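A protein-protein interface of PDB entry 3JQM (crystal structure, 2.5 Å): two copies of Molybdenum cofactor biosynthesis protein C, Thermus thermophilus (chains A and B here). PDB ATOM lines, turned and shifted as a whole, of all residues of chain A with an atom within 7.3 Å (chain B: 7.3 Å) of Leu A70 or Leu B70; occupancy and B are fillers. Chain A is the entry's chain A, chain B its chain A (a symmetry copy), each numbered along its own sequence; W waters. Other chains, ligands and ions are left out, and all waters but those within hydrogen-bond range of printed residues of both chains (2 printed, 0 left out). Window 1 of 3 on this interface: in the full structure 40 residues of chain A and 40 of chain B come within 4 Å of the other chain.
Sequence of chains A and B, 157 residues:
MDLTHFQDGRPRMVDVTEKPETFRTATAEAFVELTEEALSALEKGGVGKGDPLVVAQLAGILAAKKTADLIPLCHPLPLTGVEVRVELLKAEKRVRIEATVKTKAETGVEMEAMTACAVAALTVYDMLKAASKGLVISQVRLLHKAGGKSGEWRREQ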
ATOM      1  N   VAL A  55     -10.298  -4.789 -32.561  1.00  0.00           N
ATOM      2  CA  VAL A  55      -9.125  -5.605 -32.282  1.00  0.00           C
ATOM      3  C   VAL A  55      -8.247  -4.977 -31.208  1.00  0.00           C
ATOM      4  O   VAL A  55      -7.745  -5.683 -30.338  1.00  0.00           O
ATOM      5  CB  VAL A  55      -8.269  -5.815 -33.547  1.00  0.00           C
ATOM      6  CG1 VAL A  55      -7.084  -6.728 -33.228  1.00  0.00           C
ATOM      7  CG2 VAL A  55      -9.128  -6.395 -34.662  1.00  0.00           C
ATOM      8  N   LEU A  58      -9.431  -5.406 -27.579  1.00  0.00           N
ATOM      9  CA  LEU A  58      -9.206  -6.751 -27.073  1.00  0.00           C
ATOM     10  C   LEU A  58      -7.739  -6.933 -26.689  1.00  0.00           C
ATOM     11  O   LEU A  58      -7.421  -7.555 -25.671  1.00  0.00           O
ATOM     12  CB  LEU A  58      -9.587  -7.785 -28.131  1.00  0.00           C
ATOM     13  CG  LEU A  58     -10.657  -8.830 -27.784  1.00  0.00           C
ATOM     14  CD1 LEU A  58     -10.229 -10.179 -28.382  1.00  0.00           C
ATOM     15  CD2 LEU A  58     -10.825  -8.953 -26.270  1.00  0.00           C
ATOM     16  N   ALA A  59      -6.854  -6.387 -27.518  1.00  0.00           N
ATOM     17  CA  ALA A  59      -5.415  -6.463 -27.282  1.00  0.00           C
ATOM     18  C   ALA A  59      -5.052  -5.807 -25.959  1.00  0.00           C
ATOM     19  O   ALA A  59      -4.100  -6.222 -25.306  1.00  0.00           O
ATOM     20  CB  ALA A  59      -4.661  -5.788 -28.417  1.00  0.00           C
ATOM     21  N   GLY A  60      -5.811  -4.785 -25.564  1.00  0.00           N
ATOM     22  CA  GLY A  60      -5.550  -4.102 -24.306  1.00  0.00           C
ATOM     23  C   GLY A  60      -5.889  -4.955 -23.095  1.00  0.00           C
ATOM     24  O   GLY A  60      -5.171  -4.952 -22.091  1.00  0.00           O
ATOM     25  N   LEU A  62      -6.099  -8.324 -23.081  1.00  0.00           N
ATOM     26  CA  LEU A  62      -5.110  -9.382 -23.025  1.00  0.00           C
ATOM     27  C   LEU A  62      -3.804  -8.794 -22.497  1.00  0.00           C
ATOM     28  O   LEU A  62      -3.184  -9.339 -21.593  1.00  0.00           O
ATOM     29  CB  LEU A  62      -4.920 -10.004 -24.409  1.00  0.00           C
ATOM     30  CG  LEU A  62      -6.042 -10.978 -24.809  1.00  0.00           C
ATOM     31  CD1 LEU A  62      -5.797 -11.514 -26.209  1.00  0.00           C
ATOM     32  CD2 LEU A  62      -6.127 -12.132 -23.803  1.00  0.00           C
ATOM     33  N   ALA A  63      -3.410  -7.655 -23.045  1.00  0.00           N
ATOM     34  CA  ALA A  63      -2.185  -6.989 -22.623  1.00  0.00           C
ATOM     35  C   ALA A  63      -2.120  -6.883 -21.108  1.00  0.00           C
ATOM     36  O   ALA A  63      -1.207  -7.407 -20.484  1.00  0.00           O
ATOM     37  CB  ALA A  63      -2.104  -5.593 -23.252  1.00  0.00           C
ATOM     38  N   ALA A  64      -3.098  -6.215 -20.515  1.00  0.00           N
ATOM     39  CA  ALA A  64      -3.123  -6.041 -19.069  1.00  0.00           C
ATOM     40  C   ALA A  64      -2.829  -7.330 -18.308  1.00  0.00           C
ATOM     41  O   ALA A  64      -2.193  -7.294 -17.257  1.00  0.00           O
ATOM     42  CB  ALA A  64      -4.471  -5.470 -18.632  1.00  0.00           C
ATOM     43  N   LYS A  66      -0.903  -9.714 -19.319  1.00  0.00           N
ATOM     44  CA  LYS A  66       0.473 -10.133 -19.567  1.00  0.00           C
ATOM     45  C   LYS A  66       1.460  -9.122 -19.013  1.00  0.00           C
ATOM     46  O   LYS A  66       2.668  -9.264 -19.190  1.00  0.00           O
ATOM     47  CB  LYS A  66       0.729 -10.287 -21.067  1.00  0.00           C
ATOM     48  CG  LYS A  66      -0.197 -11.259 -21.784  1.00  0.00           C
ATOM     49  CD  LYS A  66       0.221 -11.415 -23.242  1.00  0.00           C
ATOM     50  CE  LYS A  66      -0.909 -11.979 -24.097  1.00  0.00           C
ATOM     51  NZ  LYS A  66      -1.459 -13.266 -23.580  1.00  0.00           N
ATOM     52  N   THR A  67       0.945  -8.101 -18.338  1.00  0.00           N
ATOM     53  CA  THR A  67       1.789  -7.054 -17.782  1.00  0.00           C
ATOM     54  C   THR A  67       3.055  -7.540 -17.051  1.00  0.00           C
ATOM     55  O   THR A  67       4.161  -7.163 -17.434  1.00  0.00           O
ATOM     56  CB  THR A  67       0.965  -6.113 -16.857  1.00  0.00           C
ATOM     57  OG1 THR A  67       0.005  -5.400 -17.645  1.00  0.00           O
ATOM     58  CG2 THR A  67       1.863  -5.088 -16.172  1.00  0.00           C
ATOM     59  N   ALA A  68       2.901  -8.372 -16.020  1.00  0.00           N
ATOM     60  CA  ALA A  68       4.038  -8.859 -15.235  1.00  0.00           C
ATOM     61  C   ALA A  68       5.076  -9.552 -16.101  1.00  0.00           C
ATOM     62  O   ALA A  68       6.230  -9.733 -15.705  1.00  0.00           O
ATOM     63  CB  ALA A  68       3.556  -9.809 -14.134  1.00  0.00           C
ATOM     64  N   ASP A  69       4.665  -9.925 -17.299  1.00  0.00           N
ATOM     65  CA  ASP A  69       5.560 -10.605 -18.208  1.00  0.00           C
ATOM     66  C   ASP A  69       6.385  -9.641 -19.046  1.00  0.00           C
ATOM     67  O   ASP A  69       7.392 -10.040 -19.635  1.00  0.00           O
ATOM     68  CB  ASP A  69       4.756 -11.497 -19.145  1.00  0.00           C
ATOM     69  CG  ASP A  69       5.370 -12.852 -19.301  1.00  0.00           C
ATOM     70  OD1 ASP A  69       5.225 -13.674 -18.359  1.00  0.00           O
ATOM     71  OD2 ASP A  69       6.010 -13.080 -20.354  1.00  0.00           O
ATOM     72  N   LEU A  70       5.957  -8.385 -19.108  1.00  0.00           N
ATOM     73  CA  LEU A  70       6.645  -7.395 -19.914  1.00  0.00           C
ATOM     74  C   LEU A  70       7.445  -6.379 -19.092  1.00  0.00           C
ATOM     75  O   LEU A  70       8.450  -5.858 -19.567  1.00  0.00           O
ATOM     76  CB  LEU A  70       5.623  -6.655 -20.791  1.00  0.00           C
ATOM     77  CG  LEU A  70       4.515  -7.484 -21.453  1.00  0.00           C
ATOM     78  CD1 LEU A  70       3.596  -6.575 -22.261  1.00  0.00           C
ATOM     79  CD2 LEU A  70       5.132  -8.534 -22.350  1.00  0.00           C
ATOM     80  N   ILE A  71       6.984  -6.089 -17.878  1.00  0.00           N
ATOM     81  CA  ILE A  71       7.651  -5.136 -16.992  1.00  0.00           C
ATOM     82  C   ILE A  71       8.407  -6.019 -16.004  1.00  0.00           C
ATOM     83  O   ILE A  71       7.806  -6.685 -15.164  1.00  0.00           O
ATOM     84  CB  ILE A  71       6.623  -4.213 -16.277  1.00  0.00           C
ATOM     85  CG1 ILE A  71       5.539  -3.772 -17.270  1.00  0.00           C
ATOM     86  CG2 ILE A  71       7.320  -2.991 -15.684  1.00  0.00           C
ATOM     87  CD1 ILE A  71       6.067  -3.224 -18.566  1.00  0.00           C
ATOM     88  N   PRO A  72       9.747  -6.016 -16.087  1.00  0.00           N
ATOM     89  CA  PRO A  72      10.649  -6.803 -15.242  1.00  0.00           C
ATOM     90  C   PRO A  72      10.451  -6.913 -13.730  1.00  0.00           C
ATOM     91  O   PRO A  72      10.379  -8.013 -13.195  1.00  0.00           O
ATOM     92  CB  PRO A  72      11.987  -6.128 -15.501  1.00  0.00           C
ATOM     93  CG  PRO A  72      11.894  -5.812 -16.963  1.00  0.00           C
ATOM     94  CD  PRO A  72      10.513  -5.228 -17.067  1.00  0.00           C
ATOM     95  N   LEU A  73      10.367  -5.768 -13.053  1.00  0.00           N
ATOM     96  CA  LEU A  73      10.235  -5.704 -11.592  1.00  0.00           C
ATOM     97  C   LEU A  73       8.789  -5.541 -11.128  1.00  0.00           C
ATOM     98  O   LEU A  73       8.525  -5.168  -9.988  1.00  0.00           O
ATOM     99  CB  LEU A  73      11.101  -4.578 -11.012  1.00  0.00           C
ATOM    100  CG  LEU A  73      12.508  -4.583 -11.635  1.00  0.00           C
ATOM    101  CD1 LEU A  73      13.380  -3.475 -11.039  1.00  0.00           C
ATOM    102  CD2 LEU A  73      13.145  -5.954 -11.417  1.00  0.00           C
ATOM    103  N   CYS A  74       7.855  -5.843 -12.010  1.00  0.00           N
ATOM    104  CA  CYS A  74       6.444  -5.740 -11.693  1.00  0.00           C
ATOM    105  C   CYS A  74       5.978  -6.952 -10.863  1.00  0.00           C
ATOM    106  O   CYS A  74       6.514  -8.049 -11.013  1.00  0.00           O
ATOM    107  CB  CYS A  74       5.679  -5.678 -13.010  1.00  0.00           C
ATOM    108  SG  CYS A  74       4.024  -5.088 -12.899  1.00  0.00           S
ATOM    109  N   THR A 115       0.074  -0.452 -19.316  1.00  0.00           N
ATOM    110  CA  THR A 115       0.422  -1.361 -20.416  1.00  0.00           C
ATOM    111  C   THR A 115      -0.796  -1.675 -21.286  1.00  0.00           C
ATOM    112  O   THR A 115      -0.679  -1.876 -22.496  1.00  0.00           O
ATOM    113  CB  THR A 115       1.015  -2.702 -19.895  1.00  0.00           C
ATOM    114  OG1 THR A 115       2.139  -2.439 -19.044  1.00  0.00           O
ATOM    115  CG2 THR A 115       1.482  -3.577 -21.066  1.00  0.00           C
ATOM    116  N   VAL A 119      -0.292  -1.085 -25.394  1.00  0.00           N
ATOM    117  CA  VAL A 119      -0.460  -2.204 -26.314  1.00  0.00           C
ATOM    118  C   VAL A 119      -1.683  -2.049 -27.204  1.00  0.00           C
ATOM    119  O   VAL A 119      -1.647  -2.434 -28.376  1.00  0.00           O
ATOM    120  CB  VAL A 119      -0.552  -3.543 -25.550  1.00  0.00           C
ATOM    121  CG1 VAL A 119      -1.134  -4.623 -26.453  1.00  0.00           C
ATOM    122  CG2 VAL A 119       0.830  -3.948 -25.067  1.00  0.00           C
ATOM    123  N   ALA A 120      -2.767  -1.501 -26.656  1.00  0.00           N
ATOM    124  CA  ALA A 120      -3.982  -1.272 -27.442  1.00  0.00           C
ATOM    125  C   ALA A 120      -3.611  -0.289 -28.538  1.00  0.00           C
ATOM    126  O   ALA A 120      -4.024  -0.439 -29.684  1.00  0.00           O
ATOM    127  CB  ALA A 120      -5.078  -0.687 -26.570  1.00  0.00           C
ATOM    128  N   LEU A 122      -0.518   0.275 -29.734  1.00  0.00           N
ATOM    129  CA  LEU A 122       0.358  -0.454 -30.643  1.00  0.00           C
ATOM    130  C   LEU A 122      -0.457  -1.247 -31.662  1.00  0.00           C
ATOM    131  O   LEU A 122      -0.046  -1.410 -32.812  1.00  0.00           O
ATOM    132  CB  LEU A 122       1.269  -1.411 -29.866  1.00  0.00           C
ATOM    133  CG  LEU A 122       2.448  -0.813 -29.086  1.00  0.00           C
ATOM    134  CD1 LEU A 122       3.034  -1.904 -28.216  1.00  0.00           C
ATOM    135  CD2 LEU A 122       3.521  -0.218 -30.032  1.00  0.00           C
ATOM    136  N   THR A 123      -1.616  -1.739 -31.234  1.00  0.00           N
ATOM    137  CA  THR A 123      -2.505  -2.520 -32.102  1.00  0.00           C
ATOM    138  C   THR A 123      -3.236  -1.621 -33.109  1.00  0.00           C
ATOM    139  O   THR A 123      -3.451  -2.003 -34.264  1.00  0.00           O
ATOM    140  CB  THR A 123      -3.536  -3.305 -31.253  1.00  0.00           C
ATOM    141  OG1 THR A 123      -2.826  -4.094 -30.292  1.00  0.00           O
ATOM    142  CG2 THR A 123      -4.422  -4.211 -32.138  1.00  0.00           C
ATOM    143  N   VAL B  55      17.502  -1.287 -16.789  1.00  0.00           N
ATOM    144  CA  VAL B  55      16.396  -2.235 -16.795  1.00  0.00           C
ATOM    145  C   VAL B  55      15.486  -2.027 -17.998  1.00  0.00           C
ATOM    146  O   VAL B  55      15.048  -2.998 -18.609  1.00  0.00           O
ATOM    147  CB  VAL B  55      15.544  -2.117 -15.515  1.00  0.00           C
ATOM    148  CG1 VAL B  55      14.434  -3.170 -15.531  1.00  0.00           C
ATOM    149  CG2 VAL B  55      16.431  -2.269 -14.289  1.00  0.00           C
ATOM    150  N   LEU B  58      16.741  -3.439 -21.343  1.00  0.00           N
ATOM    151  CA  LEU B  58      16.623  -4.886 -21.418  1.00  0.00           C
ATOM    152  C   LEU B  58      15.178  -5.284 -21.712  1.00  0.00           C
ATOM    153  O   LEU B  58      14.919  -6.206 -22.492  1.00  0.00           O
ATOM    154  CB  LEU B  58      17.068  -5.522 -20.103  1.00  0.00           C
ATOM    155  CG  LEU B  58      18.217  -6.539 -20.132  1.00  0.00           C
ATOM    156  CD1 LEU B  58      17.884  -7.675 -19.151  1.00  0.00           C
ATOM    157  CD2 LEU B  58      18.412  -7.100 -21.540  1.00  0.00           C
ATOM    158  N   ALA B  59      14.246  -4.582 -21.076  1.00  0.00           N
ATOM    159  CA  ALA B  59      12.819  -4.833 -21.262  1.00  0.00           C
ATOM    160  C   ALA B  59      12.423  -4.636 -22.717  1.00  0.00           C
ATOM    161  O   ALA B  59      11.513  -5.297 -23.203  1.00  0.00           O
ATOM    162  CB  ALA B  59      12.003  -3.906 -20.374  1.00  0.00           C
ATOM    163  N   GLY B  60      13.108  -3.726 -23.409  1.00  0.00           N
ATOM    164  CA  GLY B  60      12.811  -3.475 -24.812  1.00  0.00           C
ATOM    165  C   GLY B  60      13.227  -4.625 -25.714  1.00  0.00           C
ATOM    166  O   GLY B  60      12.522  -4.978 -26.664  1.00  0.00           O
ATOM    167  N   LEU B  62      13.689  -7.816 -24.716  1.00  0.00           N
ATOM    168  CA  LEU B  62      12.783  -8.912 -24.439  1.00  0.00           C
ATOM    169  C   LEU B  62      11.442  -8.610 -25.105  1.00  0.00           C
ATOM    170  O   LEU B  62      10.876  -9.447 -25.795  1.00  0.00           O
ATOM    171  CB  LEU B  62      12.624  -9.102 -22.930  1.00  0.00           C
ATOM    172  CG  LEU B  62      13.812  -9.823 -22.268  1.00  0.00           C
ATOM    173  CD1 LEU B  62      13.591  -9.930 -20.769  1.00  0.00           C
ATOM    174  CD2 LEU B  62      13.994 -11.217 -22.881  1.00  0.00           C
ATOM    175  N   ALA B  63      10.958  -7.392 -24.920  1.00  0.00           N
ATOM    176  CA  ALA B  63       9.691  -6.978 -25.508  1.00  0.00           C
ATOM    177  C   ALA B  63       9.636  -7.338 -26.984  1.00  0.00           C
ATOM    178  O   ALA B  63       8.773  -8.092 -27.411  1.00  0.00           O
ATOM    179  CB  ALA B  63       9.499  -5.468 -25.329  1.00  0.00           C
ATOM    180  N   ALA B  64      10.569  -6.808 -27.762  1.00  0.00           N
ATOM    181  CA  ALA B  64      10.597  -7.076 -29.194  1.00  0.00           C
ATOM    182  C   ALA B  64      10.409  -8.553 -29.528  1.00  0.00           C
ATOM    183  O   ALA B  64       9.784  -8.883 -30.533  1.00  0.00           O
ATOM    184  CB  ALA B  64      11.904  -6.563 -29.798  1.00  0.00           C
ATOM    185  N   LYS B  66       8.656 -10.659 -27.824  1.00  0.00           N
ATOM    186  CA  LYS B  66       7.312 -11.086 -27.446  1.00  0.00           C
ATOM    187  C   LYS B  66       6.259 -10.365 -28.266  1.00  0.00           C
ATOM    188  O   LYS B  66       5.063 -10.538 -28.042  1.00  0.00           O
ATOM    189  CB  LYS B  66       7.051 -10.800 -25.966  1.00  0.00           C
ATOM    190  CG  LYS B  66       8.039 -11.438 -25.000  1.00  0.00           C
ATOM    191  CD  LYS B  66       7.617 -11.180 -23.559  1.00  0.00           C
ATOM    192  CE  LYS B  66       8.776 -11.374 -22.587  1.00  0.00           C
ATOM    193  NZ  LYS B  66       9.428 -12.712 -22.697  1.00  0.00           N
ATOM    194  N   THR B  67       6.704  -9.559 -29.224  1.00  0.00           N
ATOM    195  CA  THR B  67       5.790  -8.795 -30.060  1.00  0.00           C
ATOM    196  C   THR B  67       4.573  -9.572 -30.596  1.00  0.00           C
ATOM    197  O   THR B  67       3.436  -9.181 -30.331  1.00  0.00           O
ATOM    198  CB  THR B  67       6.552  -8.117 -31.235  1.00  0.00           C
ATOM    199  OG1 THR B  67       7.446  -7.130 -30.708  1.00  0.00           O
ATOM    200  CG2 THR B  67       5.587  -7.416 -32.186  1.00  0.00           C
ATOM    201  N   ALA B  68       4.800 -10.661 -31.330  1.00  0.00           N
ATOM    202  CA  ALA B  68       3.712 -11.446 -31.918  1.00  0.00           C
ATOM    203  C   ALA B  68       2.719 -11.922 -30.873  1.00  0.00           C
ATOM    204  O   ALA B  68       1.587 -12.300 -31.182  1.00  0.00           O
ATOM    205  CB  ALA B  68       4.277 -12.645 -32.688  1.00  0.00           C
ATOM    206  N   ASP B  69       3.143 -11.885 -29.623  1.00  0.00           N
ATOM    207  CA  ASP B  69       2.291 -12.325 -28.541  1.00  0.00           C
ATOM    208  C   ASP B  69       1.386 -11.219 -28.022  1.00  0.00           C
ATOM    209  O   ASP B  69       0.405 -11.496 -27.329  1.00  0.00           O
ATOM    210  CB  ASP B  69       3.149 -12.831 -27.388  1.00  0.00           C
ATOM    211  CG  ASP B  69       2.636 -14.118 -26.824  1.00  0.00           C
ATOM    212  OD1 ASP B  69       2.853 -15.172 -27.478  1.00  0.00           O
ATOM    213  OD2 ASP B  69       2.003 -14.065 -25.744  1.00  0.00           O
ATOM    214  N   LEU B  70       1.719  -9.973 -28.346  1.00  0.00           N
ATOM    215  CA  LEU B  70       0.949  -8.841 -27.867  1.00  0.00           C
ATOM    216  C   LEU B  70       0.085  -8.182 -28.948  1.00  0.00           C
ATOM    217  O   LEU B  70      -0.962  -7.619 -28.640  1.00  0.00           O
ATOM    218  CB  LEU B  70       1.902  -7.797 -27.265  1.00  0.00           C
ATOM    219  CG  LEU B  70       3.062  -8.303 -26.398  1.00  0.00           C
ATOM    220  CD1 LEU B  70       3.901  -7.127 -25.911  1.00  0.00           C
ATOM    221  CD2 LEU B  70       2.515  -9.077 -25.219  1.00  0.00           C
ATOM    222  N   ILE B  71       0.537  -8.237 -30.198  1.00  0.00           N
ATOM    223  CA  ILE B  71      -0.190  -7.648 -31.321  1.00  0.00           C
ATOM    224  C   ILE B  71      -0.866  -8.842 -31.990  1.00  0.00           C
ATOM    225  O   ILE B  71      -0.208  -9.683 -32.598  1.00  0.00           O
ATOM    226  CB  ILE B  71       0.774  -6.909 -32.294  1.00  0.00           C
ATOM    227  CG1 ILE B  71       1.810  -6.110 -31.491  1.00  0.00           C
ATOM    228  CG2 ILE B  71      -0.006  -5.978 -33.220  1.00  0.00           C
ATOM    229  CD1 ILE B  71       1.228  -5.238 -30.414  1.00  0.00           C
ATOM    230  N   PRO B  72      -2.203  -8.915 -31.896  1.00  0.00           N
ATOM    231  CA  PRO B  72      -3.034  -9.985 -32.455  1.00  0.00           C
ATOM    232  C   PRO B  72      -2.811 -10.530 -33.866  1.00  0.00           C
ATOM    233  O   PRO B  72      -2.651 -11.731 -34.045  1.00  0.00           O
ATOM    234  CB  PRO B  72      -4.422  -9.365 -32.396  1.00  0.00           C
ATOM    235  CG  PRO B  72      -4.370  -8.617 -31.098  1.00  0.00           C
ATOM    236  CD  PRO B  72      -3.038  -7.928 -31.191  1.00  0.00           C
ATOM    237  N   LEU B  73      -2.805  -9.639 -34.857  1.00  0.00           N
ATOM    238  CA  LEU B  73      -2.661 -10.007 -36.270  1.00  0.00           C
ATOM    239  C   LEU B  73      -1.226  -9.884 -36.779  1.00  0.00           C
ATOM    240  O   LEU B  73      -0.978  -9.853 -37.981  1.00  0.00           O
ATOM    241  CB  LEU B  73      -3.602  -9.177 -37.151  1.00  0.00           C
ATOM    242  CG  LEU B  73      -5.013  -9.099 -36.540  1.00  0.00           C
ATOM    243  CD1 LEU B  73      -5.958  -8.291 -37.432  1.00  0.00           C
ATOM    244  CD2 LEU B  73      -5.542 -10.516 -36.329  1.00  0.00           C
ATOM    245  N   CYS B  74      -0.283  -9.836 -35.858  1.00  0.00           N
ATOM    246  CA  CYS B  74       1.121  -9.727 -36.206  1.00  0.00           C
ATOM    247  C   CYS B  74       1.685 -11.094 -36.639  1.00  0.00           C
ATOM    248  O   CYS B  74       1.231 -12.132 -36.160  1.00  0.00           O
ATOM    249  CB  CYS B  74       1.863  -9.215 -34.979  1.00  0.00           C
ATOM    250  SG  CYS B  74       3.470  -8.563 -35.281  1.00  0.00           S
ATOM    251  N   THR B 115       6.987  -1.928 -30.604  1.00  0.00           N
ATOM    252  CA  THR B 115       6.696  -2.487 -29.277  1.00  0.00           C
ATOM    253  C   THR B 115       7.924  -2.433 -28.367  1.00  0.00           C
ATOM    254  O   THR B 115       7.808  -2.268 -27.151  1.00  0.00           O
ATOM    255  CB  THR B 115       6.211  -3.963 -29.363  1.00  0.00           C
ATOM    256  OG1 THR B 115       5.080  -4.054 -30.242  1.00  0.00           O
ATOM    257  CG2 THR B 115       5.797  -4.478 -27.978  1.00  0.00           C
ATOM    258  N   VAL B 119       7.329  -0.673 -24.621  1.00  0.00           N
ATOM    259  CA  VAL B 119       7.570  -1.448 -23.409  1.00  0.00           C
ATOM    260  C   VAL B 119       8.767  -0.940 -22.622  1.00  0.00           C
ATOM    261  O   VAL B 119       8.747  -0.956 -21.387  1.00  0.00           O
ATOM    262  CB  VAL B 119       7.771  -2.943 -23.736  1.00  0.00           C
ATOM    263  CG1 VAL B 119       8.422  -3.655 -22.557  1.00  0.00           C
ATOM    264  CG2 VAL B 119       6.429  -3.578 -24.059  1.00  0.00           C
ATOM    265  N   ALA B 120       9.814  -0.504 -23.322  1.00  0.00           N
ATOM    266  CA  ALA B 120      10.999   0.042 -22.656  1.00  0.00           C
ATOM    267  C   ALA B 120      10.543   1.279 -21.902  1.00  0.00           C
ATOM    268  O   ALA B 120      10.953   1.512 -20.769  1.00  0.00           O
ATOM    269  CB  ALA B 120      12.058   0.418 -23.675  1.00  0.00           C
ATOM    270  N   LEU B 122       7.403   1.943 -20.895  1.00  0.00           N
ATOM    271  CA  LEU B 122       6.573   1.458 -19.798  1.00  0.00           C
ATOM    272  C   LEU B 122       7.434   1.072 -18.598  1.00  0.00           C
ATOM    273  O   LEU B 122       7.023   1.232 -17.447  1.00  0.00           O
ATOM    274  CB  LEU B 122       5.746   0.246 -20.240  1.00  0.00           C
ATOM    275  CG  LEU B 122       4.534   0.491 -21.151  1.00  0.00           C
ATOM    276  CD1 LEU B 122       4.041  -0.852 -21.646  1.00  0.00           C
ATOM    277  CD2 LEU B 122       3.409   1.261 -20.415  1.00  0.00           C
ATOM    278  N   THR B 123       8.631   0.562 -18.871  1.00  0.00           N
ATOM    279  CA  THR B 123       9.566   0.148 -17.818  1.00  0.00           C
ATOM    280  C   THR B 123      10.216   1.360 -17.138  1.00  0.00           C
ATOM    281  O   THR B 123      10.446   1.361 -15.924  1.00  0.00           O
ATOM    282  CB  THR B 123      10.663  -0.776 -18.404  1.00  0.00           C
ATOM    283  OG1 THR B 123      10.025  -1.869 -19.075  1.00  0.00           O
ATOM    284  CG2 THR B 123      11.604  -1.305 -17.297  1.00  0.00           C
HETATM  285  O   HOH W   1       9.765  -6.831 -21.668  1.00  0.00           O
HETATM  286  O   HOH W   2      -2.225  -8.011 -26.330  1.00  0.00           O
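Among the printed residues, pairs that only touch across the chains: Lys A66 with Asp B69, Asp A69 with Lys B66, Thr A115 with Leu B122, Leu A122 with Thr B115, Leu A70 with Leu B70, Val A119 with Leu B70, Leu A70 with Val B119, Lys A66 with Leu B70, Leu A70 with Lys B66, Val A55 with Pro B72, Pro A72 with Val B55, Pro A72 with Ala B59, Ala A59 with Pro B72, Ile A71 with Leu B122, Leu A122 with Ile B71, Thr A123 with Pro B72 and Pro A72 with Thr B123.
Ala A59 touches Pro B72, and with the chains exchanged Pro A72 touches Ala B59.
Ile A71 touches Leu B122, and with the chains exchanged Leu A122 touches Ile B71.
Pro A72 touches Thr B123, and with the chains exchanged Thr A123 touches Pro B72.
Thr A115 touches Leu B122, and with the chains exchanged Leu A122 touches Thr B115.
The backbone carbonyl oxygen (O) of Val A119 lies within hydrogen-bond range of the side-chain hydroxyl (OG1) of Thr A123, 2.8 Å away.
OG1 of Thr B123 sits at hydrogen-bond distance from O of Val B119, 2.8 Å away.
Leu B70 touches just these residues of chain A: Lys A66 (3.8 Å), Leu A70 (3.7 Å) and Val A119 (3.7 Å).
Printed residues of chain A within 4 Å of Leu B122: Ile A71 and Thr A115.
Of the printed residues of chain A, Thr B115 touches Leu A122.
Printed residues of chain B within 4 Å of Ala A59: Pro B72.
Of the printed residues of chain B, Asp A69 touches Lys B66 (3.5 Å).
Ala B120 touches none of the printed residues of chain A.
The nearest residue of chain B that does not touch Leu A70 is Ala B59 (4.1 Å).
Water W2 bridges O of Leu B70 (2.7 Å) and O of Ala A59 (2.8 Å).
Water W1 bridges the backbone carbonyl oxygen (O) of Leu A70 (2.7 Å) and the backbone carbonyl oxygen (O) of Ala B59 (2.8 Å).
Of the 21 printed residues of chain A, 11 touch a printed residue of chain B.
Printed residues of chain A that touch a printed residue of chain B: Val A55, Ala A59, Lys A66, Asp A69, Leu A70, Ile A71, Pro A72, Thr A115, Val A119, Leu A122 and Thr A123.
Of the 21 printed residues of chain B, 11 touch a printed residue of chain A.
Among the printed residues, no Asp or Glu carboxylate lies within 4 Å of a Lys or Arg side-chain nitrogen of the other chain.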
